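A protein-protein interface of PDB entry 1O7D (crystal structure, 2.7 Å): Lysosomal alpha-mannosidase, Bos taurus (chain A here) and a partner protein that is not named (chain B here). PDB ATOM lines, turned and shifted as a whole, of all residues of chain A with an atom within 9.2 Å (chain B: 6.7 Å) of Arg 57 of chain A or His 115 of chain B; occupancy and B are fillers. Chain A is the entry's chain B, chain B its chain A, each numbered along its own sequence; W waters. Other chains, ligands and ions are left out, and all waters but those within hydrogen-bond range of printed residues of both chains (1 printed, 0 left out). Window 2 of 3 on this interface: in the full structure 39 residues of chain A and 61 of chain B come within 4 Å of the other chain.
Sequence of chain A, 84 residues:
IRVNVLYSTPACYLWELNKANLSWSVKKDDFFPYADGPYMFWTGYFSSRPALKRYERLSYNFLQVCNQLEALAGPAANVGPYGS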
ATOM      1  N   PHE A  46      -7.398 -18.560  20.054  1.00  0.00           N
ATOM      2  CA  PHE A  46      -7.743 -17.154  20.124  1.00  0.00           C
ATOM      3  C   PHE A  46      -8.064 -16.669  18.726  1.00  0.00           C
ATOM      4  O   PHE A  46      -8.746 -15.667  18.549  1.00  0.00           O
ATOM      5  CB  PHE A  46      -6.597 -16.337  20.707  1.00  0.00           C
ATOM      6  CG  PHE A  46      -6.322 -16.626  22.159  1.00  0.00           C
ATOM      7  CD1 PHE A  46      -7.298 -17.198  22.968  1.00  0.00           C
ATOM      8  CD2 PHE A  46      -5.088 -16.303  22.721  1.00  0.00           C
ATOM      9  CE1 PHE A  46      -7.053 -17.446  24.301  1.00  0.00           C
ATOM     10  CE2 PHE A  46      -4.835 -16.549  24.060  1.00  0.00           C
ATOM     11  CZ  PHE A  46      -5.819 -17.120  24.849  1.00  0.00           C
ATOM     12  N   PRO A  50     -11.473 -18.136  11.947  1.00  0.00           N
ATOM     13  CA  PRO A  50     -11.776 -16.713  11.729  1.00  0.00           C
ATOM     14  C   PRO A  50     -13.192 -16.446  11.217  1.00  0.00           C
ATOM     15  O   PRO A  50     -13.896 -15.567  11.720  1.00  0.00           O
ATOM     16  CB  PRO A  50     -10.727 -16.289  10.706  1.00  0.00           C
ATOM     17  CG  PRO A  50      -9.593 -17.207  10.982  1.00  0.00           C
ATOM     18  CD  PRO A  50     -10.270 -18.529  11.198  1.00  0.00           C
ATOM     19  N   ALA A  51     -13.587 -17.206  10.200  1.00  0.00           N
ATOM     20  CA  ALA A  51     -14.899 -17.072   9.589  1.00  0.00           C
ATOM     21  C   ALA A  51     -16.013 -17.148  10.611  1.00  0.00           C
ATOM     22  O   ALA A  51     -16.779 -16.202  10.768  1.00  0.00           O
ATOM     23  CB  ALA A  51     -15.093 -18.139   8.553  1.00  0.00           C
ATOM     24  N   LEU A  52     -16.111 -18.273  11.307  1.00  0.00           N
ATOM     25  CA  LEU A  52     -17.156 -18.414  12.303  1.00  0.00           C
ATOM     26  C   LEU A  52     -17.081 -17.309  13.342  1.00  0.00           C
ATOM     27  O   LEU A  52     -18.090 -16.686  13.673  1.00  0.00           O
ATOM     28  CB  LEU A  52     -17.064 -19.767  13.003  1.00  0.00           C
ATOM     29  CG  LEU A  52     -18.216 -20.046  13.972  1.00  0.00           C
ATOM     30  CD1 LEU A  52     -19.556 -19.856  13.278  1.00  0.00           C
ATOM     31  CD2 LEU A  52     -18.085 -21.450  14.486  1.00  0.00           C
ATOM     32  N   LYS A  53     -15.878 -17.067  13.856  1.00  0.00           N
ATOM     33  CA  LYS A  53     -15.708 -16.037  14.865  1.00  0.00           C
ATOM     34  C   LYS A  53     -16.354 -14.727  14.419  1.00  0.00           C
ATOM     35  O   LYS A  53     -17.039 -14.080  15.201  1.00  0.00           O
ATOM     36  CB  LYS A  53     -14.221 -15.845  15.184  1.00  0.00           C
ATOM     37  CG  LYS A  53     -13.712 -16.744  16.313  1.00  0.00           C
ATOM     38  CD  LYS A  53     -12.183 -16.697  16.458  1.00  0.00           C
ATOM     39  CE  LYS A  53     -11.687 -17.347  17.762  1.00  0.00           C
ATOM     40  NZ  LYS A  53     -11.833 -18.822  17.816  1.00  0.00           N
ATOM     41  N   ARG A  54     -16.162 -14.361  13.157  1.00  0.00           N
ATOM     42  CA  ARG A  54     -16.737 -13.137  12.607  1.00  0.00           C
ATOM     43  C   ARG A  54     -18.249 -13.243  12.396  1.00  0.00           C
ATOM     44  O   ARG A  54     -18.978 -12.274  12.595  1.00  0.00           O
ATOM     45  CB  ARG A  54     -16.052 -12.801  11.276  1.00  0.00           C
ATOM     46  CG  ARG A  54     -16.675 -11.642  10.512  1.00  0.00           C
ATOM     47  CD  ARG A  54     -16.649 -10.345  11.311  1.00  0.00           C
ATOM     48  NE  ARG A  54     -17.582  -9.355  10.772  1.00  0.00           N
ATOM     49  CZ  ARG A  54     -17.789  -8.153  11.303  1.00  0.00           C
ATOM     50  NH1 ARG A  54     -17.122  -7.783  12.390  1.00  0.00           N
ATOM     51  NH2 ARG A  54     -18.670  -7.328  10.751  1.00  0.00           N
ATOM     52  N   TYR A  55     -18.708 -14.422  11.988  1.00  0.00           N
ATOM     53  CA  TYR A  55     -20.125 -14.656  11.741  1.00  0.00           C
ATOM     54  C   TYR A  55     -20.924 -14.415  13.007  1.00  0.00           C
ATOM     55  O   TYR A  55     -22.034 -13.896  12.962  1.00  0.00           O
ATOM     56  CB  TYR A  55     -20.358 -16.094  11.277  1.00  0.00           C
ATOM     57  CG  TYR A  55     -21.765 -16.373  10.800  1.00  0.00           C
ATOM     58  CD1 TYR A  55     -22.216 -17.675  10.622  1.00  0.00           C
ATOM     59  CD2 TYR A  55     -22.638 -15.335  10.493  1.00  0.00           C
ATOM     60  CE1 TYR A  55     -23.489 -17.933  10.153  1.00  0.00           C
ATOM     61  CE2 TYR A  55     -23.913 -15.586  10.024  1.00  0.00           C
ATOM     62  CZ  TYR A  55     -24.329 -16.885   9.856  1.00  0.00           C
ATOM     63  OH  TYR A  55     -25.591 -17.135   9.383  1.00  0.00           O
ATOM     64  N   GLU A  56     -20.350 -14.799  14.141  1.00  0.00           N
ATOM     65  CA  GLU A  56     -21.018 -14.629  15.415  1.00  0.00           C
ATOM     66  C   GLU A  56     -20.993 -13.188  15.879  1.00  0.00           C
ATOM     67  O   GLU A  56     -22.048 -12.629  16.174  1.00  0.00           O
ATOM     68  CB  GLU A  56     -20.395 -15.550  16.472  1.00  0.00           C
ATOM     69  CG  GLU A  56     -20.833 -15.298  17.908  1.00  0.00           C
ATOM     70  CD  GLU A  56     -19.962 -14.252  18.599  1.00  0.00           C
ATOM     71  OE1 GLU A  56     -18.946 -13.847  17.988  1.00  0.00           O
ATOM     72  OE2 GLU A  56     -20.271 -13.834  19.737  1.00  0.00           O
ATOM     73  N   ARG A  57     -19.819 -12.562  15.927  1.00  0.00           N
ATOM     74  CA  ARG A  57     -19.782 -11.183  16.402  1.00  0.00           C
ATOM     75  C   ARG A  57     -20.638 -10.275  15.536  1.00  0.00           C
ATOM     76  O   ARG A  57     -20.956  -9.156  15.925  1.00  0.00           O
ATOM     77  CB  ARG A  57     -18.358 -10.610  16.475  1.00  0.00           C
ATOM     78  CG  ARG A  57     -18.354  -9.363  17.352  1.00  0.00           C
ATOM     79  CD  ARG A  57     -17.202  -8.397  17.169  1.00  0.00           C
ATOM     80  NE  ARG A  57     -15.963  -8.733  17.884  1.00  0.00           N
ATOM     81  CZ  ARG A  57     -15.850  -9.552  18.929  1.00  0.00           C
ATOM     82  NH1 ARG A  57     -16.908 -10.179  19.444  1.00  0.00           N
ATOM     83  NH2 ARG A  57     -14.656  -9.733  19.475  1.00  0.00           N
ATOM     84  N   LEU A  58     -21.007 -10.769  14.362  1.00  0.00           N
ATOM     85  CA  LEU A  58     -21.834 -10.019  13.433  1.00  0.00           C
ATOM     86  C   LEU A  58     -23.288 -10.283  13.759  1.00  0.00           C
ATOM     87  O   LEU A  58     -24.117  -9.374  13.719  1.00  0.00           O
ATOM     88  CB  LEU A  58     -21.540 -10.453  12.004  1.00  0.00           C
ATOM     89  CG  LEU A  58     -22.415  -9.886  10.886  1.00  0.00           C
ATOM     90  CD1 LEU A  58     -22.264  -8.377  10.817  1.00  0.00           C
ATOM     91  CD2 LEU A  58     -22.015 -10.549   9.566  1.00  0.00           C
ATOM     92  N   SER A  59     -23.600 -11.534  14.083  1.00  0.00           N
ATOM     93  CA  SER A  59     -24.969 -11.885  14.430  1.00  0.00           C
ATOM     94  C   SER A  59     -25.376 -11.095  15.687  1.00  0.00           C
ATOM     95  O   SER A  59     -26.568 -10.794  15.906  1.00  0.00           O
ATOM     96  CB  SER A  59     -25.090 -13.392  14.673  1.00  0.00           C
ATOM     97  OG  SER A  59     -24.865 -14.125  13.488  1.00  0.00           O
ATOM     98  N   TYR A  60     -24.382 -10.753  16.507  1.00  0.00           N
ATOM     99  CA  TYR A  60     -24.641  -9.975  17.708  1.00  0.00           C
ATOM    100  C   TYR A  60     -25.187  -8.594  17.304  1.00  0.00           C
ATOM    101  O   TYR A  60     -26.269  -8.183  17.733  1.00  0.00           O
ATOM    102  CB  TYR A  60     -23.360  -9.794  18.529  1.00  0.00           C
ATOM    103  CG  TYR A  60     -23.556  -8.893  19.740  1.00  0.00           C
ATOM    104  CD1 TYR A  60     -24.138  -9.378  20.918  1.00  0.00           C
ATOM    105  CD2 TYR A  60     -23.192  -7.543  19.691  1.00  0.00           C
ATOM    106  CE1 TYR A  60     -24.347  -8.541  22.008  1.00  0.00           C
ATOM    107  CE2 TYR A  60     -23.400  -6.702  20.775  1.00  0.00           C
ATOM    108  CZ  TYR A  60     -23.975  -7.203  21.931  1.00  0.00           C
ATOM    109  OH  TYR A  60     -24.164  -6.363  23.005  1.00  0.00           O
ATOM    110  N   ASN A  61     -24.421  -7.890  16.474  1.00  0.00           N
ATOM    111  CA  ASN A  61     -24.788  -6.568  15.995  1.00  0.00           C
ATOM    112  C   ASN A  61     -26.185  -6.641  15.433  1.00  0.00           C
ATOM    113  O   ASN A  61     -26.988  -5.732  15.615  1.00  0.00           O
ATOM    114  CB  ASN A  61     -23.829  -6.130  14.888  1.00  0.00           C
ATOM    115  CG  ASN A  61     -23.938  -4.657  14.567  1.00  0.00           C
ATOM    116  OD1 ASN A  61     -23.191  -4.126  13.744  1.00  0.00           O
ATOM    117  ND2 ASN A  61     -24.864  -3.984  15.223  1.00  0.00           N
ATOM    118  N   PHE A  62     -26.458  -7.753  14.758  1.00  0.00           N
ATOM    119  CA  PHE A  62     -27.736  -7.987  14.109  1.00  0.00           C
ATOM    120  C   PHE A  62     -28.887  -8.241  15.077  1.00  0.00           C
ATOM    121  O   PHE A  62     -29.944  -7.619  14.958  1.00  0.00           O
ATOM    122  CB  PHE A  62     -27.607  -9.155  13.120  1.00  0.00           C
ATOM    123  CG  PHE A  62     -28.796  -9.319  12.211  1.00  0.00           C
ATOM    124  CD1 PHE A  62     -29.095  -8.354  11.260  1.00  0.00           C
ATOM    125  CD2 PHE A  62     -29.643 -10.416  12.338  1.00  0.00           C
ATOM    126  CE1 PHE A  62     -30.224  -8.477  10.450  1.00  0.00           C
ATOM    127  CE2 PHE A  62     -30.779 -10.554  11.530  1.00  0.00           C
ATOM    128  CZ  PHE A  62     -31.073  -9.584  10.589  1.00  0.00           C
ATOM    129  N   LEU A  63     -28.692  -9.155  16.020  1.00  0.00           N
ATOM    130  CA  LEU A  63     -29.729  -9.462  16.997  1.00  0.00           C
ATOM    131  C   LEU A  63     -30.122  -8.174  17.736  1.00  0.00           C
ATOM    132  O   LEU A  63     -31.296  -7.929  18.021  1.00  0.00           O
ATOM    133  CB  LEU A  63     -29.201 -10.485  18.005  1.00  0.00           C
ATOM    134  CG  LEU A  63     -30.138 -11.415  18.788  1.00  0.00           C
ATOM    135  CD1 LEU A  63     -29.458 -11.733  20.105  1.00  0.00           C
ATOM    136  CD2 LEU A  63     -31.483 -10.789  19.041  1.00  0.00           C
ATOM    137  N   GLN A  64     -29.120  -7.360  18.044  1.00  0.00           N
ATOM    138  CA  GLN A  64     -29.323  -6.097  18.736  1.00  0.00           C
ATOM    139  C   GLN A  64     -30.300  -5.226  17.965  1.00  0.00           C
ATOM    140  O   GLN A  64     -31.319  -4.796  18.498  1.00  0.00           O
ATOM    141  CB  GLN A  64     -28.002  -5.357  18.858  1.00  0.00           C
ATOM    142  CG  GLN A  64     -27.778  -4.823  20.230  1.00  0.00           C
ATOM    143  CD  GLN A  64     -27.368  -5.905  21.193  1.00  0.00           C
ATOM    144  OE1 GLN A  64     -27.948  -7.003  21.217  1.00  0.00           O
ATOM    145  NE2 GLN A  64     -26.363  -5.604  22.008  1.00  0.00           N
ATOM    146  N   ASP B 110     -17.242 -19.566  26.831  1.00  0.00           N
ATOM    147  CA  ASP B 110     -15.791 -19.449  26.785  1.00  0.00           C
ATOM    148  C   ASP B 110     -15.411 -18.059  27.284  1.00  0.00           C
ATOM    149  O   ASP B 110     -16.233 -17.154  27.253  1.00  0.00           O
ATOM    150  CB  ASP B 110     -15.310 -19.618  25.351  1.00  0.00           C
ATOM    151  CG  ASP B 110     -13.859 -19.324  25.211  1.00  0.00           C
ATOM    152  OD1 ASP B 110     -13.045 -20.122  25.744  1.00  0.00           O
ATOM    153  OD2 ASP B 110     -13.544 -18.288  24.592  1.00  0.00           O
ATOM    154  N   THR B 113     -12.703 -15.519  23.657  1.00  0.00           N
ATOM    155  CA  THR B 113     -13.239 -14.971  22.431  1.00  0.00           C
ATOM    156  C   THR B 113     -14.645 -14.389  22.496  1.00  0.00           C
ATOM    157  O   THR B 113     -15.139 -13.851  21.509  1.00  0.00           O
ATOM    158  CB  THR B 113     -13.193 -16.034  21.349  1.00  0.00           C
ATOM    159  OG1 THR B 113     -13.868 -17.214  21.810  1.00  0.00           O
ATOM    160  CG2 THR B 113     -11.733 -16.363  21.006  1.00  0.00           C
ATOM    161  N   THR B 114     -15.290 -14.477  23.646  1.00  0.00           N
ATOM    162  CA  THR B 114     -16.635 -13.943  23.785  1.00  0.00           C
ATOM    163  C   THR B 114     -16.677 -12.448  24.065  1.00  0.00           C
ATOM    164  O   THR B 114     -15.774 -11.895  24.682  1.00  0.00           O
ATOM    165  CB  THR B 114     -17.368 -14.637  24.897  1.00  0.00           C
ATOM    166  OG1 THR B 114     -16.525 -14.668  26.055  1.00  0.00           O
ATOM    167  CG2 THR B 114     -17.724 -16.046  24.484  1.00  0.00           C
ATOM    168  N   HIS B 115     -17.746 -11.810  23.599  1.00  0.00           N
ATOM    169  CA  HIS B 115     -17.982 -10.381  23.758  1.00  0.00           C
ATOM    170  C   HIS B 115     -18.754 -10.232  25.053  1.00  0.00           C
ATOM    171  O   HIS B 115     -19.715 -10.959  25.254  1.00  0.00           O
ATOM    172  CB  HIS B 115     -18.829  -9.891  22.579  1.00  0.00           C
ATOM    173  CG  HIS B 115     -19.252  -8.461  22.684  1.00  0.00           C
ATOM    174  ND1 HIS B 115     -18.355  -7.416  22.692  1.00  0.00           N
ATOM    175  CD2 HIS B 115     -20.479  -7.907  22.790  1.00  0.00           C
ATOM    176  CE1 HIS B 115     -19.012  -6.276  22.801  1.00  0.00           C
ATOM    177  NE2 HIS B 115     -20.302  -6.546  22.860  1.00  0.00           N
ATOM    178  N   TYR B 116     -18.369  -9.306  25.927  1.00  0.00           N
ATOM    179  CA  TYR B 116     -19.081  -9.167  27.201  1.00  0.00           C
ATOM    180  C   TYR B 116     -20.609  -9.071  27.047  1.00  0.00           C
ATOM    181  O   TYR B 116     -21.361  -9.631  27.844  1.00  0.00           O
ATOM    182  CB  TYR B 116     -18.550  -7.957  27.975  1.00  0.00           C
ATOM    183  CG  TYR B 116     -19.132  -6.639  27.547  1.00  0.00           C
ATOM    184  CD1 TYR B 116     -20.362  -6.200  28.043  1.00  0.00           C
ATOM    185  CD2 TYR B 116     -18.482  -5.851  26.617  1.00  0.00           C
ATOM    186  CE1 TYR B 116     -20.928  -5.002  27.611  1.00  0.00           C
ATOM    187  CE2 TYR B 116     -19.033  -4.659  26.179  1.00  0.00           C
ATOM    188  CZ  TYR B 116     -20.256  -4.233  26.670  1.00  0.00           C
ATOM    189  OH  TYR B 116     -20.801  -3.044  26.200  1.00  0.00           O
ATOM    190  N   GLY B 117     -21.061  -8.379  26.004  1.00  0.00           N
ATOM    191  CA  GLY B 117     -22.483  -8.212  25.781  1.00  0.00           C
ATOM    192  C   GLY B 117     -23.164  -9.502  25.409  1.00  0.00           C
ATOM    193  O   GLY B 117     -24.292  -9.747  25.804  1.00  0.00           O
ATOM    194  N   ALA B 118     -22.471 -10.331  24.641  1.00  0.00           N
ATOM    195  CA  ALA B 118     -23.019 -11.597  24.207  1.00  0.00           C
ATOM    196  C   ALA B 118     -23.067 -12.580  25.367  1.00  0.00           C
ATOM    197  O   ALA B 118     -23.978 -13.400  25.462  1.00  0.00           O
ATOM    198  CB  ALA B 118     -22.184 -12.134  23.082  1.00  0.00           C
ATOM    199  N   ILE B 119     -22.080 -12.494  26.248  1.00  0.00           N
ATOM    200  CA  ILE B 119     -22.028 -13.357  27.415  1.00  0.00           C
ATOM    201  C   ILE B 119     -23.249 -13.079  28.287  1.00  0.00           C
ATOM    202  O   ILE B 119     -23.804 -13.972  28.910  1.00  0.00           O
ATOM    203  CB  ILE B 119     -20.754 -13.075  28.234  1.00  0.00           C
ATOM    204  CG1 ILE B 119     -19.532 -13.521  27.438  1.00  0.00           C
ATOM    205  CG2 ILE B 119     -20.811 -13.779  29.581  1.00  0.00           C
ATOM    206  CD1 ILE B 119     -18.222 -13.003  28.008  1.00  0.00           C
ATOM    207  N   ILE B 120     -23.666 -11.825  28.330  1.00  0.00           N
ATOM    208  CA  ILE B 120     -24.817 -11.457  29.131  1.00  0.00           C
ATOM    209  C   ILE B 120     -26.122 -11.995  28.538  1.00  0.00           C
ATOM    210  O   ILE B 120     -26.941 -12.580  29.252  1.00  0.00           O
ATOM    211  CB  ILE B 120     -24.894  -9.932  29.283  1.00  0.00           C
ATOM    212  CG1 ILE B 120     -23.585  -9.421  29.890  1.00  0.00           C
ATOM    213  CG2 ILE B 120     -26.079  -9.544  30.158  1.00  0.00           C
ATOM    214  CD1 ILE B 120     -23.519  -7.904  30.010  1.00  0.00           C
ATOM    215  N   LEU B 158     -18.467  -9.629  35.518  1.00  0.00           N
ATOM    216  CA  LEU B 158     -19.824  -9.904  35.077  1.00  0.00           C
ATOM    217  C   LEU B 158     -20.585 -10.761  36.068  1.00  0.00           C
ATOM    218  O   LEU B 158     -21.729 -10.448  36.416  1.00  0.00           O
ATOM    219  CB  LEU B 158     -19.801 -10.580  33.702  1.00  0.00           C
ATOM    220  CG  LEU B 158     -20.022  -9.715  32.445  1.00  0.00           C
ATOM    221  CD1 LEU B 158     -19.435  -8.318  32.587  1.00  0.00           C
ATOM    222  CD2 LEU B 158     -19.410 -10.432  31.271  1.00  0.00           C
HETATM  223  O   HOH W   1     -19.006 -13.475  21.896  1.00  0.00           O
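The side-chain hydroxyl of Tyr 60 of chain A lies within hydrogen-bond range of the side-chain amide nitrogen of Gln 64 of chain A (2.5 Å). OD2 of Asp 110 of chain B sits at hydrogen-bond distance from OG1 of Thr 113 of chain B.
Among the printed residues, pairs that only touch across the chains: Phe 46 of chain A with Thr 113 of chain B, Lys 53 of chain A with Thr 113 of chain B, Arg 57 of chain A with His 115 of chain B, Tyr 60 of chain A with His 115 of chain B, Tyr 60 of chain A with Gly 117 of chain B and Tyr 60 of chain A with Ala 118 of chain B.
Of the printed residues of chain B, Phe 46 of chain A touches Thr 113. Printed residues of chain B within 4 Å of Lys 53 of chain A: Thr 113 (3.4 Å). Of chain B, only His 115 (3.7 Å) comes within 4 Å of Arg 57 of chain A. Ser 59 of chain A touches none of the printed residues of chain B. Of the printed residues of chain B, Tyr 60 of chain A touches His 115, Gly 117 and Ala 118. Leu 63 of chain A touches none of the printed residues of chain B. No residue of chain A comes within 4 Å of Thr 114 of chain B. Ala 118 of chain B touches one residue of chain A. The nearest residue of chain B that does not touch Arg 57 of chain A is Thr 113 of chain B (4.6 Å). The nearest residue of chain A that does not touch His 115 of chain B is Glu 56 of chain A (5.0 Å). The nearest printed residue of chain A that does not touch Thr 113 of chain B is Arg 57 of chain A (4.6 Å).
Hydrophobic or aromatic side chains of chain B within 4 Å of the printed part of chain A: His 115. Hydrophobic or aromatic side chains of chain A within 4 Å of the printed part of chain B: Tyr 60. Among the printed residues, 6 pairs touch across the chains.
Water W1 lies within hydrogen-bond range of the side-chain carboxylate of Glu 56 of chain A (2.5 Å) and the backbone NH of His 115 of chain B (2.7 Å).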
